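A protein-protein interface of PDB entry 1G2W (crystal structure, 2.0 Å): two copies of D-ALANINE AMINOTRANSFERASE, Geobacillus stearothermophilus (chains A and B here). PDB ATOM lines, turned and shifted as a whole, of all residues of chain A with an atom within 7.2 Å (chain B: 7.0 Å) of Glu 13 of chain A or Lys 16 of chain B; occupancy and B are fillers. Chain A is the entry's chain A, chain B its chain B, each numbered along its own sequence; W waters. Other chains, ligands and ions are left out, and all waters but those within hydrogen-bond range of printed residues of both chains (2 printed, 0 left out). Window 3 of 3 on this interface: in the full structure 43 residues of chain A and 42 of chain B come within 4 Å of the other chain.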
ATOM      1  N   GLY A   1      18.574   7.179  22.962  1.00  0.00           N
ATOM      2  CA  GLY A   1      17.271   6.769  23.547  1.00  0.00           C
ATOM      3  C   GLY A   1      16.543   7.907  24.238  1.00  0.00           C
ATOM      4  O   GLY A   1      16.770   9.084  23.940  1.00  0.00           O
ATOM      5  N   TYR A   2      15.661   7.557  25.168  1.00  0.00           N
ATOM      6  CA  TYR A   2      14.892   8.551  25.897  1.00  0.00           C
ATOM      7  C   TYR A   2      15.262   8.569  27.372  1.00  0.00           C
ATOM      8  O   TYR A   2      15.624   7.544  27.950  1.00  0.00           O
ATOM      9  CB  TYR A   2      13.394   8.285  25.740  1.00  0.00           C
ATOM     10  CG  TYR A   2      12.899   8.444  24.318  1.00  0.00           C
ATOM     11  CD1 TYR A   2      13.154   7.467  23.354  1.00  0.00           C
ATOM     12  CD2 TYR A   2      12.203   9.591  23.928  1.00  0.00           C
ATOM     13  CE1 TYR A   2      12.728   7.628  22.035  1.00  0.00           C
ATOM     14  CE2 TYR A   2      11.776   9.761  22.613  1.00  0.00           C
ATOM     15  CZ  TYR A   2      12.040   8.778  21.673  1.00  0.00           C
ATOM     16  OH  TYR A   2      11.609   8.947  20.378  1.00  0.00           O
ATOM     17  N   THR A   3      15.169   9.749  27.973  1.00  0.00           N
ATOM     18  CA  THR A   3      15.491   9.919  29.380  1.00  0.00           C
ATOM     19  C   THR A   3      14.299  10.505  30.101  1.00  0.00           C
ATOM     20  O   THR A   3      13.600  11.362  29.567  1.00  0.00           O
ATOM     21  CB  THR A   3      16.674  10.885  29.579  1.00  0.00           C
ATOM     22  OG1 THR A   3      17.867  10.306  29.036  1.00  0.00           O
ATOM     23  CG2 THR A   3      16.877  11.182  31.058  1.00  0.00           C
ATOM     24  N   VAL A  10      11.986  12.551  27.411  1.00  0.00           N
ATOM     25  CA  VAL A  10      12.596  13.317  26.334  1.00  0.00           C
ATOM     26  C   VAL A  10      13.792  12.610  25.717  1.00  0.00           C
ATOM     27  O   VAL A  10      14.325  11.662  26.288  1.00  0.00           O
ATOM     28  CB  VAL A  10      13.045  14.706  26.854  1.00  0.00           C
ATOM     29  CG1 VAL A  10      11.853  15.438  27.462  1.00  0.00           C
ATOM     30  CG2 VAL A  10      14.133  14.549  27.901  1.00  0.00           C
ATOM     31  N   LYS A  11      14.206  13.066  24.540  1.00  0.00           N
ATOM     32  CA  LYS A  11      15.364  12.480  23.879  1.00  0.00           C
ATOM     33  C   LYS A  11      16.561  12.873  24.734  1.00  0.00           C
ATOM     34  O   LYS A  11      16.628  14.008  25.205  1.00  0.00           O
ATOM     35  CB  LYS A  11      15.510  13.048  22.465  1.00  0.00           C
ATOM     36  CG  LYS A  11      14.323  12.746  21.559  1.00  0.00           C
ATOM     37  CD  LYS A  11      14.432  13.471  20.225  1.00  0.00           C
ATOM     38  CE  LYS A  11      13.270  13.117  19.310  1.00  0.00           C
ATOM     39  NZ  LYS A  11      13.256  11.663  18.977  1.00  0.00           N
ATOM     40  N   ASP A  12      17.493  11.942  24.944  1.00  0.00           N
ATOM     41  CA  ASP A  12      18.680  12.202  25.760  1.00  0.00           C
ATOM     42  C   ASP A  12      19.344  13.542  25.441  1.00  0.00           C
ATOM     43  O   ASP A  12      19.793  14.250  26.336  1.00  0.00           O
ATOM     44  CB  ASP A  12      19.718  11.090  25.576  1.00  0.00           C
ATOM     45  CG  ASP A  12      19.147   9.703  25.818  1.00  0.00           C
ATOM     46  OD1 ASP A  12      18.332   9.545  26.746  1.00  0.00           O
ATOM     47  OD2 ASP A  12      19.530   8.769  25.085  1.00  0.00           O
ATOM     48  N   GLU A  13      19.407  13.878  24.161  1.00  0.00           N
ATOM     49  CA  GLU A  13      20.020  15.123  23.699  1.00  0.00           C
ATOM     50  C   GLU A  13      19.429  16.388  24.327  1.00  0.00           C
ATOM     51  O   GLU A  13      20.122  17.390  24.483  1.00  0.00           O
ATOM     52  CB  GLU A  13      19.881  15.234  22.178  1.00  0.00           C
ATOM     53  CG  GLU A  13      20.541  14.125  21.373  1.00  0.00           C
ATOM     54  CD  GLU A  13      19.983  12.739  21.677  1.00  0.00           C
ATOM     55  OE1 GLU A  13      18.742  12.579  21.709  1.00  0.00           O
ATOM     56  OE2 GLU A  13      20.792  11.805  21.872  1.00  0.00           O
ATOM     57  N   GLU A  14      18.149  16.346  24.680  1.00  0.00           N
ATOM     58  CA  GLU A  14      17.475  17.513  25.243  1.00  0.00           C
ATOM     59  C   GLU A  14      17.724  17.767  26.726  1.00  0.00           C
ATOM     60  O   GLU A  14      17.484  18.881  27.211  1.00  0.00           O
ATOM     61  CB  GLU A  14      15.961  17.411  25.029  1.00  0.00           C
ATOM     62  CG  GLU A  14      15.512  17.337  23.583  1.00  0.00           C
ATOM     63  CD  GLU A  14      13.992  17.388  23.442  1.00  0.00           C
ATOM     64  OE1 GLU A  14      13.487  17.098  22.334  1.00  0.00           O
ATOM     65  OE2 GLU A  14      13.303  17.723  24.432  1.00  0.00           O
ATOM     66  N   VAL A  15      18.205  16.755  27.444  1.00  0.00           N
ATOM     67  CA  VAL A  15      18.423  16.902  28.879  1.00  0.00           C
ATOM     68  C   VAL A  15      19.595  17.789  29.249  1.00  0.00           C
ATOM     69  O   VAL A  15      20.706  17.605  28.763  1.00  0.00           O
ATOM     70  CB  VAL A  15      18.602  15.528  29.557  1.00  0.00           C
ATOM     71  CG1 VAL A  15      18.943  15.710  31.033  1.00  0.00           C
ATOM     72  CG2 VAL A  15      17.322  14.727  29.419  1.00  0.00           C
ATOM     73  N   LYS A  16      19.342  18.757  30.119  1.00  0.00           N
ATOM     74  CA  LYS A  16      20.396  19.662  30.551  1.00  0.00           C
ATOM     75  C   LYS A  16      20.364  19.854  32.065  1.00  0.00           C
ATOM     76  O   LYS A  16      19.316  20.128  32.649  1.00  0.00           O
ATOM     77  CB  LYS A  16      20.257  21.009  29.837  1.00  0.00           C
ATOM     78  CG  LYS A  16      20.353  20.894  28.319  1.00  0.00           C
ATOM     79  CD  LYS A  16      20.200  22.234  27.607  1.00  0.00           C
ATOM     80  CE  LYS A  16      21.398  23.157  27.821  1.00  0.00           C
ATOM     81  NZ  LYS A  16      21.528  23.637  29.227  1.00  0.00           N
ATOM     82  N   ILE A  17      21.526  19.690  32.686  1.00  0.00           N
ATOM     83  CA  ILE A  17      21.677  19.838  34.127  1.00  0.00           C
ATOM     84  C   ILE A  17      22.241  21.225  34.410  1.00  0.00           C
ATOM     85  O   ILE A  17      23.160  21.670  33.729  1.00  0.00           O
ATOM     86  CB  ILE A  17      22.656  18.779  34.697  1.00  0.00           C
ATOM     87  CG1 ILE A  17      22.267  17.377  34.203  1.00  0.00           C
ATOM     88  CG2 ILE A  17      22.647  18.822  36.215  1.00  0.00           C
ATOM     89  CD1 ILE A  17      20.828  16.982  34.503  1.00  0.00           C
ATOM     90  N   ASP A  18      21.697  21.894  35.419  1.00  0.00           N
ATOM     91  CA  ASP A  18      22.145  23.234  35.789  1.00  0.00           C
ATOM     92  C   ASP A  18      23.356  23.149  36.703  1.00  0.00           C
ATOM     93  O   ASP A  18      23.423  22.273  37.566  1.00  0.00           O
ATOM     94  CB  ASP A  18      21.017  23.987  36.493  1.00  0.00           C
ATOM     95  CG  ASP A  18      21.301  25.477  36.619  1.00  0.00           C
ATOM     96  OD1 ASP A  18      22.078  25.885  37.515  1.00  0.00           O
ATOM     97  OD2 ASP A  18      20.746  26.239  35.800  1.00  0.00           O
ATOM     98  N   TYR A  24      24.700  18.474  41.869  1.00  0.00           N
ATOM     99  CA  TYR A  24      25.989  18.689  41.221  1.00  0.00           C
ATOM    100  C   TYR A  24      26.989  19.397  42.130  1.00  0.00           C
ATOM    101  O   TYR A  24      28.194  19.247  41.967  1.00  0.00           O
ATOM    102  CB  TYR A  24      25.795  19.511  39.938  1.00  0.00           C
ATOM    103  CG  TYR A  24      26.984  19.515  38.996  1.00  0.00           C
ATOM    104  CD1 TYR A  24      27.497  18.326  38.486  1.00  0.00           C
ATOM    105  CD2 TYR A  24      27.567  20.711  38.579  1.00  0.00           C
ATOM    106  CE1 TYR A  24      28.553  18.324  37.584  1.00  0.00           C
ATOM    107  CE2 TYR A  24      28.627  20.721  37.675  1.00  0.00           C
ATOM    108  CZ  TYR A  24      29.112  19.525  37.180  1.00  0.00           C
ATOM    109  OH  TYR A  24      30.145  19.523  36.278  1.00  0.00           O
ATOM    110  N   TRP B   5      34.009  27.720  31.868  1.00  0.00           N
ATOM    111  CA  TRP B   5      33.636  26.367  31.502  1.00  0.00           C
ATOM    112  C   TRP B   5      34.821  25.690  30.829  1.00  0.00           C
ATOM    113  O   TRP B   5      35.166  25.997  29.684  1.00  0.00           O
ATOM    114  CB  TRP B   5      32.418  26.392  30.581  1.00  0.00           C
ATOM    115  CG  TRP B   5      31.871  25.038  30.278  1.00  0.00           C
ATOM    116  CD1 TRP B   5      31.921  23.928  31.082  1.00  0.00           C
ATOM    117  CD2 TRP B   5      31.155  24.652  29.107  1.00  0.00           C
ATOM    118  NE1 TRP B   5      31.279  22.876  30.478  1.00  0.00           N
ATOM    119  CE2 TRP B   5      30.797  23.291  29.264  1.00  0.00           C
ATOM    120  CE3 TRP B   5      30.778  25.320  27.935  1.00  0.00           C
ATOM    121  CZ2 TRP B   5      30.080  22.588  28.291  1.00  0.00           C
ATOM    122  CZ3 TRP B   5      30.064  24.621  26.969  1.00  0.00           C
ATOM    123  CH2 TRP B   5      29.724  23.268  27.154  1.00  0.00           C
ATOM    124  N   ASP B  12      26.746  32.259  30.726  1.00  0.00           N
ATOM    125  CA  ASP B  12      26.113  31.182  31.485  1.00  0.00           C
ATOM    126  C   ASP B  12      25.249  30.283  30.601  1.00  0.00           C
ATOM    127  O   ASP B  12      25.303  29.058  30.698  1.00  0.00           O
ATOM    128  CB  ASP B  12      25.242  31.749  32.615  1.00  0.00           C
ATOM    129  CG  ASP B  12      25.972  32.768  33.472  1.00  0.00           C
ATOM    130  OD1 ASP B  12      27.205  32.656  33.614  1.00  0.00           O
ATOM    131  OD2 ASP B  12      25.306  33.676  34.020  1.00  0.00           O
ATOM    132  N   GLU B  13      24.462  30.909  29.733  1.00  0.00           N
ATOM    133  CA  GLU B  13      23.549  30.213  28.825  1.00  0.00           C
ATOM    134  C   GLU B  13      24.147  29.113  27.941  1.00  0.00           C
ATOM    135  O   GLU B  13      23.429  28.218  27.502  1.00  0.00           O
ATOM    136  CB  GLU B  13      22.863  31.248  27.929  1.00  0.00           C
ATOM    137  CG  GLU B  13      23.851  32.073  27.111  1.00  0.00           C
ATOM    138  CD  GLU B  13      23.199  33.224  26.370  1.00  0.00           C
ATOM    139  OE1 GLU B  13      22.681  34.149  27.034  1.00  0.00           O
ATOM    140  OE2 GLU B  13      23.210  33.205  25.120  1.00  0.00           O
ATOM    141  N   GLU B  14      25.447  29.177  27.675  1.00  0.00           N
ATOM    142  CA  GLU B  14      26.095  28.190  26.812  1.00  0.00           C
ATOM    143  C   GLU B  14      26.581  26.927  27.534  1.00  0.00           C
ATOM    144  O   GLU B  14      26.903  25.925  26.894  1.00  0.00           O
ATOM    145  CB  GLU B  14      27.284  28.829  26.094  1.00  0.00           C
ATOM    146  CG  GLU B  14      26.962  30.110  25.334  1.00  0.00           C
ATOM    147  CD  GLU B  14      28.190  30.689  24.645  1.00  0.00           C
ATOM    148  OE1 GLU B  14      28.704  30.041  23.705  1.00  0.00           O
ATOM    149  OE2 GLU B  14      28.645  31.784  25.051  1.00  0.00           O
ATOM    150  N   VAL B  15      26.641  26.982  28.859  1.00  0.00           N
ATOM    151  CA  VAL B  15      27.106  25.847  29.650  1.00  0.00           C
ATOM    152  C   VAL B  15      26.126  24.671  29.642  1.00  0.00           C
ATOM    153  O   VAL B  15      24.927  24.847  29.861  1.00  0.00           O
ATOM    154  CB  VAL B  15      27.364  26.267  31.124  1.00  0.00           C
ATOM    155  CG1 VAL B  15      27.731  25.048  31.961  1.00  0.00           C
ATOM    156  CG2 VAL B  15      28.478  27.291  31.182  1.00  0.00           C
ATOM    157  N   LYS B  16      26.642  23.473  29.383  1.00  0.00           N
ATOM    158  CA  LYS B  16      25.803  22.280  29.377  1.00  0.00           C
ATOM    159  C   LYS B  16      26.443  21.170  30.214  1.00  0.00           C
ATOM    160  O   LYS B  16      27.543  20.714  29.908  1.00  0.00           O
ATOM    161  CB  LYS B  16      25.578  21.780  27.943  1.00  0.00           C
ATOM    162  CG  LYS B  16      24.688  20.541  27.871  1.00  0.00           C
ATOM    163  CD  LYS B  16      24.306  20.166  26.445  1.00  0.00           C
ATOM    164  CE  LYS B  16      23.327  18.991  26.439  1.00  0.00           C
ATOM    165  NZ  LYS B  16      22.836  18.655  25.073  1.00  0.00           N
ATOM    166  N   ILE B  17      25.756  20.753  31.276  1.00  0.00           N
ATOM    167  CA  ILE B  17      26.250  19.683  32.142  1.00  0.00           C
ATOM    168  C   ILE B  17      25.534  18.380  31.762  1.00  0.00           C
ATOM    169  O   ILE B  17      24.305  18.347  31.675  1.00  0.00           O
ATOM    170  CB  ILE B  17      25.953  19.969  33.637  1.00  0.00           C
ATOM    171  CG1 ILE B  17      26.464  21.360  34.038  1.00  0.00           C
ATOM    172  CG2 ILE B  17      26.596  18.891  34.502  1.00  0.00           C
ATOM    173  CD1 ILE B  17      27.954  21.530  33.935  1.00  0.00           C
ATOM    174  N   ASP B  18      26.298  17.316  31.541  1.00  0.00           N
ATOM    175  CA  ASP B  18      25.718  16.019  31.173  1.00  0.00           C
ATOM    176  C   ASP B  18      25.187  15.273  32.402  1.00  0.00           C
ATOM    177  O   ASP B  18      25.736  15.403  33.494  1.00  0.00           O
ATOM    178  CB  ASP B  18      26.762  15.140  30.485  1.00  0.00           C
ATOM    179  CG  ASP B  18      26.145  13.914  29.837  1.00  0.00           C
ATOM    180  OD1 ASP B  18      25.695  14.020  28.681  1.00  0.00           O
ATOM    181  OD2 ASP B  18      26.089  12.848  30.482  1.00  0.00           O
ATOM    182  N   ASP B  21      27.817  13.250  34.242  1.00  0.00           N
ATOM    183  CA  ASP B  21      29.013  13.944  34.690  1.00  0.00           C
ATOM    184  C   ASP B  21      29.197  13.260  36.046  1.00  0.00           C
ATOM    185  O   ASP B  21      28.242  13.180  36.827  1.00  0.00           O
ATOM    186  CB  ASP B  21      28.728  15.437  34.894  1.00  0.00           C
ATOM    187  CG  ASP B  21      29.954  16.213  35.356  1.00  0.00           C
ATOM    188  OD1 ASP B  21      30.609  15.767  36.328  1.00  0.00           O
ATOM    189  OD2 ASP B  21      30.261  17.273  34.754  1.00  0.00           O
ATOM    190  N   THR B  95      32.715  13.255  32.348  1.00  0.00           N
ATOM    191  CA  THR B  95      31.495  12.595  31.893  1.00  0.00           C
ATOM    192  C   THR B  95      31.850  11.239  31.302  1.00  0.00           C
ATOM    193  O   THR B  95      32.730  11.135  30.448  1.00  0.00           O
ATOM    194  CB  THR B  95      30.795  13.439  30.819  1.00  0.00           C
ATOM    195  OG1 THR B  95      30.458  14.713  31.374  1.00  0.00           O
ATOM    196  CG2 THR B  95      29.522  12.753  30.325  1.00  0.00           C
ATOM    197  N   VAL B 110      35.785  18.077  34.032  1.00  0.00           N
ATOM    198  CA  VAL B 110      34.909  19.193  33.709  1.00  0.00           C
ATOM    199  C   VAL B 110      35.167  20.274  34.750  1.00  0.00           C
ATOM    200  O   VAL B 110      35.115  20.018  35.962  1.00  0.00           O
ATOM    201  CB  VAL B 110      33.418  18.773  33.726  1.00  0.00           C
ATOM    202  CG1 VAL B 110      32.517  19.991  33.579  1.00  0.00           C
ATOM    203  CG2 VAL B 110      33.146  17.788  32.575  1.00  0.00           C
ATOM    204  N   ILE B 112      34.156  24.097  36.175  1.00  0.00           N
ATOM    205  CA  ILE B 112      33.104  25.095  36.236  1.00  0.00           C
ATOM    206  C   ILE B 112      33.451  26.156  37.278  1.00  0.00           C
ATOM    207  O   ILE B 112      33.851  25.837  38.402  1.00  0.00           O
ATOM    208  CB  ILE B 112      31.750  24.460  36.626  1.00  0.00           C
ATOM    209  CG1 ILE B 112      31.235  23.576  35.486  1.00  0.00           C
ATOM    210  CG2 ILE B 112      30.736  25.551  36.979  1.00  0.00           C
ATOM    211  CD1 ILE B 112      30.846  24.345  34.233  1.00  0.00           C
HETATM  212  O   HOH W   1      32.531  20.765  37.129  1.00  0.00           O
HETATM  213  O   HOH W   2      22.650  14.854  29.680  1.00  0.00           O
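The side-chain amino group (NZ) of Lys 16 of chain B is in hydrogen-bond range of the backbone carbonyl oxygen (O) of Glu 13 of chain A (3.1 Å). The backbone NH of Ile 17 of chain A lies within hydrogen-bond range of the backbone carbonyl oxygen of Ile 17 of chain B (3.2 Å). The side-chain carboxylate (OD2) of Asp 21 of chain B lies within hydrogen-bond range of the side-chain hydroxyl (OH) of Tyr 24 of chain A (2.7 Å).
Among the printed residues, merely in contact across the chains: Tyr 24 of chain A with Val 110 of chain B, Lys 16 of chain A with Val 15 of chain B, Tyr 24 of chain A with Ile 17 of chain B and Val 15 of chain A with Lys 16 of chain B.
Lys 11 of chain A touches none of the printed residues of chain B. Of chain B, only Lys 16 (3.1 Å) comes within 4 Å of Glu 13 of chain A. Glu 14 of chain A touches none of the printed residues of chain B. Of the printed residues of chain B, Val 15 of chain A touches Lys 16 (3.8 Å). Printed residues of chain B within 4 Å of Lys 16 of chain A: Val 15 (3.7 Å). Of the printed residues of chain B, Ile 17 of chain A touches Ile 17 (3.2 Å). Printed residues of chain A within 4 Å of Lys 16 of chain B: Glu 13 and Val 15. Of the printed residues of chain A, Ile 17 of chain B touches Ile 17 and Tyr 24. Of the printed residues of chain A, Asp 21 of chain B touches Tyr 24 (2.7 Å).
Printed residues of chain A that touch a printed residue of chain B: Glu 13, Val 15, Lys 16, Ile 17 and Tyr 24. Hydrophobic or aromatic side chains of chain A within 4 Å of the printed part of chain B: Ile 17 and Tyr 24. Of the 12 printed residues of chain B, 5 touch a printed residue of chain A.
Glu 13 of chain A touches Lys 16 of chain B, but with the chains exchanged Lys 16 of chain A does not touch Glu 13 of chain B (5.3 Å). Val 15 of chain A touches Lys 16 of chain B, and with the chains exchanged Lys 16 of chain A touches Val 15 of chain B. Ile 17 of chain A touches its own counterpart, Ile 17 of chain B. Positions printed for both chains: 12, 13, 14, 15, 16, 17 and 18. Of the 7 pairs that touch across the chains among the printed residues, 3 have their exchanged pair printed and touching as well.
Water W1 lies within hydrogen-bond range of OH of Tyr 24 of chain A (2.8 Å) and O of Val 110 of chain B (2.9 Å). Water W2 bridges the side-chain carboxylate (OD1) of Asp 18 of chain B (3.3 Å) and the backbone carbonyl oxygen (O) of Val 15 of chain A (3.5 Å).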
